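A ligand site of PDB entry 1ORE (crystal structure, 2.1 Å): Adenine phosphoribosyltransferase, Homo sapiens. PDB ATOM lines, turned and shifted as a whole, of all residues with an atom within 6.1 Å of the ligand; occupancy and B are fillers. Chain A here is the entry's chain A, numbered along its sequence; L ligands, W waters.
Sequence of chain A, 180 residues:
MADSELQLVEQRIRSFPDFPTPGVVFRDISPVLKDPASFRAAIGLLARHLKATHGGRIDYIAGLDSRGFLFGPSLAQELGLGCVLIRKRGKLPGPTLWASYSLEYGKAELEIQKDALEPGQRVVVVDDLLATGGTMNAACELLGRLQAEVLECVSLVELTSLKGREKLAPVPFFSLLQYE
Water W5 bridges O2 of the ligand (2.5 Å) and N of Met 136 (3.0 Å).
Water W2 lies within hydrogen-bond range of an oxygen (O7) of the ligand (2.9 Å) and the guanidinium group of Arg 67 (3.3 Å).
Water W3 lies within hydrogen-bond range of the side-chain carboxylate of Asp 127 (2.6 Å), the backbone NH of Arg 67 (3.0 Å), an oxygen (O6) of the ligand (3.3 Å) and the backbone carbonyl oxygen of Asp 65 (3.3 Å).
O2 of the ligand lies within hydrogen-bond range of N of Gly 133 (2.9 Å).
The backbone NH of Thr 132 lies within hydrogen-bond range of an oxygen (O3) of the ligand (2.9 Å).
An oxygen (O1) of the ligand lies within hydrogen-bond range of the backbone NH (N) of Gly 134 (3.5 Å).
The backbone NH (N) of Arg 27 sits at hydrogen-bond distance from a nitrogen (N4) of the ligand.
The backbone carbonyl oxygen of Val 25 is in hydrogen-bond range of a nitrogen (N3) of the ligand, at 2.9 Å.
The backbone NH (N) of Ala 131 sits at hydrogen-bond distance from an oxygen (O2) of the ligand, 3.0 Å away.
OG1 of Thr 132 lies within hydrogen-bond range of O3 of the ligand (2.6 Å).
OD2 of Asp 128 lies within hydrogen-bond range of O7 of the ligand (2.5 Å).
OG1 of Thr 135 lies within hydrogen-bond range of O1 of the ligand, at 2.7 Å.
The backbone NH of Thr 135 lies within hydrogen-bond range of an oxygen (O1) of the ligand (2.9 Å).
An oxygen (O7) of the ligand sits at hydrogen-bond distance from the guanidinium group (NH2) of Arg 67 (3.0 Å).
The side-chain carboxylate of Asp 127 sits at hydrogen-bond distance from an oxygen (O6) of the ligand (2.7 Å).
Merely in contact with the ligand: Phe 26 (3.5 Å), Leu 129 (3.5 Å) and Leu 159 (3.7 Å).
Hydrophobic or aromatic side chains that line the ligand: Phe 26, Leu 129, Ala 131 and Leu 159.
The nearest printed residue that does not touch the ligand is Val 24 (4.1 Å).
NE of Arg 67 is in salt-bridge range of OD1 of Asp 128 (2.8 Å).
N of Leu 159 is in hydrogen-bond range of O of Leu 130 (2.9 Å).
N of Gly 134 is in hydrogen-bond range of OG1 of Thr 132 (3.2 Å).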
ATOM      1  N   PHE A  19      36.250 -14.838  25.617  1.00  0.00           N
ATOM      2  CA  PHE A  19      35.575 -15.232  24.385  1.00  0.00           C
ATOM      3  C   PHE A  19      34.280 -14.460  24.223  1.00  0.00           C
ATOM      4  O   PHE A  19      33.490 -14.385  25.159  1.00  0.00           O
ATOM      5  CB  PHE A  19      35.296 -16.723  24.343  1.00  0.00           C
ATOM      6  CG  PHE A  19      34.713 -17.137  23.036  1.00  0.00           C
ATOM      7  CD1 PHE A  19      33.328 -17.177  22.869  1.00  0.00           C
ATOM      8  CD2 PHE A  19      35.537 -17.392  21.949  1.00  0.00           C
ATOM      9  CE1 PHE A  19      32.763 -17.529  21.622  1.00  0.00           C
ATOM     10  CE2 PHE A  19      34.999 -17.731  20.712  1.00  0.00           C
ATOM     11  CZ  PHE A  19      33.597 -17.799  20.549  1.00  0.00           C
ATOM     12  N   VAL A  24      35.847 -10.563  28.126  1.00  0.00           N
ATOM     13  CA  VAL A  24      34.434 -10.952  28.047  1.00  0.00           C
ATOM     14  C   VAL A  24      34.271 -12.419  28.521  1.00  0.00           C
ATOM     15  O   VAL A  24      34.948 -13.323  28.015  1.00  0.00           O
ATOM     16  CB  VAL A  24      33.823 -10.713  26.628  1.00  0.00           C
ATOM     17  CG1 VAL A  24      32.403 -11.263  26.501  1.00  0.00           C
ATOM     18  CG2 VAL A  24      33.769  -9.213  26.291  1.00  0.00           C
ATOM     19  N   VAL A  25      33.380 -12.641  29.481  1.00  0.00           N
ATOM     20  CA  VAL A  25      33.073 -13.994  29.940  1.00  0.00           C
ATOM     21  C   VAL A  25      31.862 -14.502  29.156  1.00  0.00           C
ATOM     22  O   VAL A  25      30.749 -13.999  29.304  1.00  0.00           O
ATOM     23  CB  VAL A  25      32.822 -14.055  31.459  1.00  0.00           C
ATOM     24  CG1 VAL A  25      32.505 -15.471  31.924  1.00  0.00           C
ATOM     25  CG2 VAL A  25      34.080 -13.497  32.217  1.00  0.00           C
ATOM     26  N   PHE A  26      32.093 -15.525  28.337  1.00  0.00           N
ATOM     27  CA  PHE A  26      31.032 -16.112  27.571  1.00  0.00           C
ATOM     28  C   PHE A  26      30.238 -17.048  28.464  1.00  0.00           C
ATOM     29  O   PHE A  26      30.795 -17.955  29.080  1.00  0.00           O
ATOM     30  CB  PHE A  26      31.623 -16.852  26.384  1.00  0.00           C
ATOM     31  CG  PHE A  26      30.594 -17.385  25.419  1.00  0.00           C
ATOM     32  CD1 PHE A  26      30.129 -16.582  24.357  1.00  0.00           C
ATOM     33  CD2 PHE A  26      30.104 -18.673  25.542  1.00  0.00           C
ATOM     34  CE1 PHE A  26      29.164 -17.073  23.425  1.00  0.00           C
ATOM     35  CE2 PHE A  26      29.139 -19.172  24.631  1.00  0.00           C
ATOM     36  CZ  PHE A  26      28.660 -18.355  23.565  1.00  0.00           C
ATOM     37  N   ARG A  27      28.923 -16.866  28.494  1.00  0.00           N
ATOM     38  CA  ARG A  27      28.017 -17.762  29.213  1.00  0.00           C
ATOM     39  C   ARG A  27      27.329 -18.714  28.218  1.00  0.00           C
ATOM     40  O   ARG A  27      26.591 -18.274  27.352  1.00  0.00           O
ATOM     41  CB  ARG A  27      26.961 -16.947  29.947  1.00  0.00           C
ATOM     42  CG  ARG A  27      27.525 -15.829  30.807  1.00  0.00           C
ATOM     43  CD  ARG A  27      28.518 -16.295  31.866  1.00  0.00           C
ATOM     44  NE  ARG A  27      28.951 -15.191  32.714  1.00  0.00           N
ATOM     45  CZ  ARG A  27      29.454 -15.334  33.950  1.00  0.00           C
ATOM     46  NH1 ARG A  27      29.616 -16.543  34.551  1.00  0.00           N
ATOM     47  NH2 ARG A  27      29.726 -14.239  34.615  1.00  0.00           N
ATOM     48  N   ASP A  28      27.652 -19.990  28.323  1.00  0.00           N
ATOM     49  CA  ASP A  28      27.202 -21.037  27.440  1.00  0.00           C
ATOM     50  C   ASP A  28      25.982 -21.774  28.033  1.00  0.00           C
ATOM     51  O   ASP A  28      26.091 -22.420  29.093  1.00  0.00           O
ATOM     52  CB  ASP A  28      28.392 -21.949  27.183  1.00  0.00           C
ATOM     53  CG  ASP A  28      28.091 -23.151  26.294  1.00  0.00           C
ATOM     54  OD1 ASP A  28      27.120 -23.145  25.550  1.00  0.00           O
ATOM     55  OD2 ASP A  28      28.784 -24.188  26.330  1.00  0.00           O
ATOM     56  N   LEU A  64      14.920 -15.009  18.750  1.00  0.00           N
ATOM     57  CA  LEU A  64      16.086 -14.357  18.136  1.00  0.00           C
ATOM     58  C   LEU A  64      17.164 -15.355  17.659  1.00  0.00           C
ATOM     59  O   LEU A  64      17.541 -16.298  18.339  1.00  0.00           O
ATOM     60  CB  LEU A  64      16.747 -13.355  19.101  1.00  0.00           C
ATOM     61  CG  LEU A  64      15.824 -12.259  19.612  1.00  0.00           C
ATOM     62  CD1 LEU A  64      16.589 -11.124  20.277  1.00  0.00           C
ATOM     63  CD2 LEU A  64      14.874 -11.723  18.559  1.00  0.00           C
ATOM     64  N   ASP A  65      17.608 -15.139  16.431  1.00  0.00           N
ATOM     65  CA  ASP A  65      18.581 -15.998  15.763  1.00  0.00           C
ATOM     66  C   ASP A  65      19.913 -15.772  16.487  1.00  0.00           C
ATOM     67  O   ASP A  65      20.261 -14.605  16.735  1.00  0.00           O
ATOM     68  CB  ASP A  65      18.631 -15.486  14.321  1.00  0.00           C
ATOM     69  CG  ASP A  65      19.592 -16.255  13.429  1.00  0.00           C
ATOM     70  OD1 ASP A  65      19.694 -15.805  12.268  1.00  0.00           O
ATOM     71  OD2 ASP A  65      20.252 -17.298  13.780  1.00  0.00           O
ATOM     72  N   ARG A  67      20.535 -18.392  19.086  1.00  0.00           N
ATOM     73  CA  ARG A  67      20.283 -19.084  20.370  1.00  0.00           C
ATOM     74  C   ARG A  67      18.889 -18.900  20.934  1.00  0.00           C
ATOM     75  O   ARG A  67      18.413 -19.777  21.641  1.00  0.00           O
ATOM     76  CB  ARG A  67      21.368 -18.751  21.382  1.00  0.00           C
ATOM     77  CG  ARG A  67      22.708 -19.297  20.899  1.00  0.00           C
ATOM     78  CD  ARG A  67      23.815 -19.366  21.899  1.00  0.00           C
ATOM     79  NE  ARG A  67      24.377 -18.061  22.266  1.00  0.00           N
ATOM     80  CZ  ARG A  67      25.420 -17.472  21.683  1.00  0.00           C
ATOM     81  NH1 ARG A  67      26.027 -18.011  20.653  1.00  0.00           N
ATOM     82  NH2 ARG A  67      25.853 -16.303  22.141  1.00  0.00           N
ATOM     83  N   LEU A 103      27.002  -0.137  17.857  1.00  0.00           N
ATOM     84  CA  LEU A 103      27.086   0.064  19.306  1.00  0.00           C
ATOM     85  C   LEU A 103      28.537   0.077  19.739  1.00  0.00           C
ATOM     86  O   LEU A 103      29.427  -0.277  18.958  1.00  0.00           O
ATOM     87  CB  LEU A 103      26.329  -1.024  20.040  1.00  0.00           C
ATOM     88  CG  LEU A 103      24.938  -1.316  19.421  1.00  0.00           C
ATOM     89  CD1 LEU A 103      24.501  -2.753  19.581  1.00  0.00           C
ATOM     90  CD2 LEU A 103      23.918  -0.355  19.970  1.00  0.00           C
ATOM     91  N   ALA A 108      24.411  -4.803  16.316  1.00  0.00           N
ATOM     92  CA  ALA A 108      23.214  -5.639  16.312  1.00  0.00           C
ATOM     93  C   ALA A 108      22.484  -5.416  14.979  1.00  0.00           C
ATOM     94  O   ALA A 108      21.949  -4.326  14.723  1.00  0.00           O
ATOM     95  CB  ALA A 108      22.331  -5.279  17.466  1.00  0.00           C
ATOM     96  N   ASP A 127      15.465 -14.539  23.934  1.00  0.00           N
ATOM     97  CA  ASP A 127      16.850 -14.883  23.565  1.00  0.00           C
ATOM     98  C   ASP A 127      17.473 -15.619  24.735  1.00  0.00           C
ATOM     99  O   ASP A 127      16.895 -15.655  25.858  1.00  0.00           O
ATOM    100  CB  ASP A 127      17.632 -13.599  23.267  1.00  0.00           C
ATOM    101  CG  ASP A 127      18.763 -13.807  22.222  1.00  0.00           C
ATOM    102  OD1 ASP A 127      19.013 -14.950  21.734  1.00  0.00           O
ATOM    103  OD2 ASP A 127      19.466 -12.854  21.858  1.00  0.00           O
ATOM    104  N   ASP A 128      18.642 -16.205  24.509  1.00  0.00           N
ATOM    105  CA  ASP A 128      19.347 -16.904  25.592  1.00  0.00           C
ATOM    106  C   ASP A 128      19.820 -15.954  26.693  1.00  0.00           C
ATOM    107  O   ASP A 128      19.691 -16.298  27.868  1.00  0.00           O
ATOM    108  CB  ASP A 128      20.468 -17.803  25.079  1.00  0.00           C
ATOM    109  CG  ASP A 128      21.635 -17.044  24.447  1.00  0.00           C
ATOM    110  OD1 ASP A 128      22.760 -17.595  24.524  1.00  0.00           O
ATOM    111  OD2 ASP A 128      21.530 -15.921  23.895  1.00  0.00           O
ATOM    112  N   LEU A 129      20.230 -14.752  26.297  1.00  0.00           N
ATOM    113  CA  LEU A 129      20.990 -13.877  27.188  1.00  0.00           C
ATOM    114  C   LEU A 129      20.831 -12.410  26.784  1.00  0.00           C
ATOM    115  O   LEU A 129      20.856 -12.059  25.626  1.00  0.00           O
ATOM    116  CB  LEU A 129      22.491 -14.242  27.133  1.00  0.00           C
ATOM    117  CG  LEU A 129      23.494 -13.502  28.030  1.00  0.00           C
ATOM    118  CD1 LEU A 129      24.684 -14.449  28.407  1.00  0.00           C
ATOM    119  CD2 LEU A 129      24.048 -12.245  27.368  1.00  0.00           C
ATOM    120  N   LEU A 130      20.685 -11.583  27.808  1.00  0.00           N
ATOM    121  CA  LEU A 130      20.667 -10.139  27.736  1.00  0.00           C
ATOM    122  C   LEU A 130      21.969  -9.577  28.320  1.00  0.00           C
ATOM    123  O   LEU A 130      22.346  -9.851  29.458  1.00  0.00           O
ATOM    124  CB  LEU A 130      19.477  -9.571  28.525  1.00  0.00           C
ATOM    125  CG  LEU A 130      19.396  -8.042  28.466  1.00  0.00           C
ATOM    126  CD1 LEU A 130      18.873  -7.621  27.102  1.00  0.00           C
ATOM    127  CD2 LEU A 130      18.520  -7.504  29.583  1.00  0.00           C
ATOM    128  N   ALA A 131      22.640  -8.770  27.519  1.00  0.00           N
ATOM    129  CA  ALA A 131      23.847  -8.076  27.903  1.00  0.00           C
ATOM    130  C   ALA A 131      23.531  -6.587  27.784  1.00  0.00           C
ATOM    131  O   ALA A 131      22.806  -6.072  28.636  1.00  0.00           O
ATOM    132  CB  ALA A 131      25.045  -8.550  27.024  1.00  0.00           C
ATOM    133  N   THR A 132      24.026  -5.887  26.752  1.00  0.00           N
ATOM    134  CA  THR A 132      23.770  -4.433  26.610  1.00  0.00           C
ATOM    135  C   THR A 132      22.307  -4.136  26.265  1.00  0.00           C
ATOM    136  O   THR A 132      21.828  -3.030  26.547  1.00  0.00           O
ATOM    137  CB  THR A 132      24.617  -3.761  25.508  1.00  0.00           C
ATOM    138  OG1 THR A 132      24.311  -4.319  24.219  1.00  0.00           O
ATOM    139  CG2 THR A 132      26.156  -3.949  25.702  1.00  0.00           C
ATOM    140  N   GLY A 133      21.594  -5.111  25.694  1.00  0.00           N
ATOM    141  CA  GLY A 133      20.249  -4.874  25.155  1.00  0.00           C
ATOM    142  C   GLY A 133      20.169  -4.403  23.700  1.00  0.00           C
ATOM    143  O   GLY A 133      19.063  -4.210  23.157  1.00  0.00           O
ATOM    144  N   GLY A 134      21.319  -4.238  23.050  1.00  0.00           N
ATOM    145  CA  GLY A 134      21.392  -3.854  21.667  1.00  0.00           C
ATOM    146  C   GLY A 134      20.582  -4.743  20.748  1.00  0.00           C
ATOM    147  O   GLY A 134      19.851  -4.268  19.884  1.00  0.00           O
ATOM    148  N   THR A 135      20.706  -6.036  20.954  1.00  0.00           N
ATOM    149  CA  THR A 135      20.020  -7.019  20.128  1.00  0.00           C
ATOM    150  C   THR A 135      18.522  -7.010  20.336  1.00  0.00           C
ATOM    151  O   THR A 135      17.759  -6.929  19.379  1.00  0.00           O
ATOM    152  CB  THR A 135      20.621  -8.400  20.421  1.00  0.00           C
ATOM    153  OG1 THR A 135      22.018  -8.392  20.117  1.00  0.00           O
ATOM    154  CG2 THR A 135      20.044  -9.452  19.494  1.00  0.00           C
ATOM    155  N   MET A 136      18.078  -7.107  21.588  1.00  0.00           N
ATOM    156  CA  MET A 136      16.652  -7.101  21.893  1.00  0.00           C
ATOM    157  C   MET A 136      16.036  -5.753  21.531  1.00  0.00           C
ATOM    158  O   MET A 136      14.889  -5.676  21.109  1.00  0.00           O
ATOM    159  CB  MET A 136      16.403  -7.436  23.376  1.00  0.00           C
ATOM    160  CG  MET A 136      16.010  -8.884  23.645  1.00  0.00           C
ATOM    161  SD  MET A 136      16.107  -9.340  25.381  1.00  0.00           S
ATOM    162  CE  MET A 136      16.013 -11.055  25.271  1.00  0.00           C
ATOM    163  N   LEU A 159      23.235 -10.156  32.228  1.00  0.00           N
ATOM    164  CA  LEU A 159      24.473  -9.557  32.716  1.00  0.00           C
ATOM    165  C   LEU A 159      24.164  -8.173  33.210  1.00  0.00           C
ATOM    166  O   LEU A 159      24.105  -7.215  32.428  1.00  0.00           O
ATOM    167  CB  LEU A 159      25.551  -9.509  31.617  1.00  0.00           C
ATOM    168  CG  LEU A 159      25.775 -10.837  30.873  1.00  0.00           C
ATOM    169  CD1 LEU A 159      26.952 -10.750  29.924  1.00  0.00           C
ATOM    170  CD2 LEU A 159      25.961 -11.999  31.885  1.00  0.00           C
ATOM    171  N   LEU A 162      25.757  -4.551  32.540  1.00  0.00           N
ATOM    172  CA  LEU A 162      25.635  -3.955  31.210  1.00  0.00           C
ATOM    173  C   LEU A 162      24.338  -3.165  30.921  1.00  0.00           C
ATOM    174  O   LEU A 162      24.179  -2.611  29.853  1.00  0.00           O
ATOM    175  CB  LEU A 162      25.899  -5.022  30.137  1.00  0.00           C
ATOM    176  CG  LEU A 162      27.298  -5.688  30.284  1.00  0.00           C
ATOM    177  CD1 LEU A 162      27.520  -6.770  29.249  1.00  0.00           C
ATOM    178  CD2 LEU A 162      28.425  -4.623  30.194  1.00  0.00           C
HETATM  179  P1  LIG L   1      23.486  -7.692  23.698  1.00  0.00           P
HETATM  180  O1  LIG L   1      22.940  -7.257  22.358  1.00  0.00           O
HETATM  181  O2  LIG L   1      22.293  -7.709  24.696  1.00  0.00           O
HETATM  182  O3  LIG L   1      24.703  -6.849  24.078  1.00  0.00           O
HETATM  183  O4  LIG L   1      24.052  -9.184  23.586  1.00  0.00           O
HETATM  184  C1  LIG L   1      23.109 -10.242  23.643  1.00  0.00           C
HETATM  185  C2  LIG L   1      23.275 -11.114  22.403  1.00  0.00           C
HETATM  186  O5  LIG L   1      24.641 -11.474  22.133  1.00  0.00           O
HETATM  187  C3  LIG L   1      22.559 -12.445  22.617  1.00  0.00           C
HETATM  188  O6  LIG L   1      22.157 -12.896  21.329  1.00  0.00           O
HETATM  189  C4  LIG L   1      23.623 -13.327  23.279  1.00  0.00           C
HETATM  190  O7  LIG L   1      23.467 -14.705  22.902  1.00  0.00           O
HETATM  191  C5  LIG L   1      24.964 -12.693  22.810  1.00  0.00           C
HETATM  192  N1  LIG L   1      25.867 -12.410  23.938  1.00  0.00           N
HETATM  193  C6  LIG L   1      26.337 -11.184  24.378  1.00  0.00           C
HETATM  194  N2  LIG L   1      27.161 -11.374  25.437  1.00  0.00           N
HETATM  195  C7  LIG L   1      27.258 -12.709  25.676  1.00  0.00           C
HETATM  196  C8  LIG L   1      27.982 -13.433  26.616  1.00  0.00           C
HETATM  197  N3  LIG L   1      28.778 -12.827  27.524  1.00  0.00           N
HETATM  198  N4  LIG L   1      27.900 -14.825  26.570  1.00  0.00           N
HETATM  199  C9  LIG L   1      27.074 -15.445  25.662  1.00  0.00           C
HETATM  200  N5  LIG L   1      26.364 -14.715  24.747  1.00  0.00           N
HETATM  201  C10 LIG L   1      26.482 -13.364  24.731  1.00  0.00           C
HETATM  202  O   HOH W   1      26.695  -9.459  20.826  1.00  0.00           O
HETATM  203  O   HOH W   2      23.454 -15.384  20.051  1.00  0.00           O
HETATM  204  O   HOH W   3      20.765 -15.497  19.912  1.00  0.00           O
HETATM  205  O   HOH W   4      24.707  -5.869  20.686  1.00  0.00           O
HETATM  206  O   HOH W   5      19.930  -7.900  23.842  1.00  0.00           O
HETATM  207  O   HOH W   6      28.954  -9.560  27.229  1.00  0.00           O
HETATM  208  O   HOH W   7      27.157  -7.615  23.696  1.00  0.00           O
HETATM  209  O   HOH W   8      22.849 -12.157  18.780  1.00  0.00           O
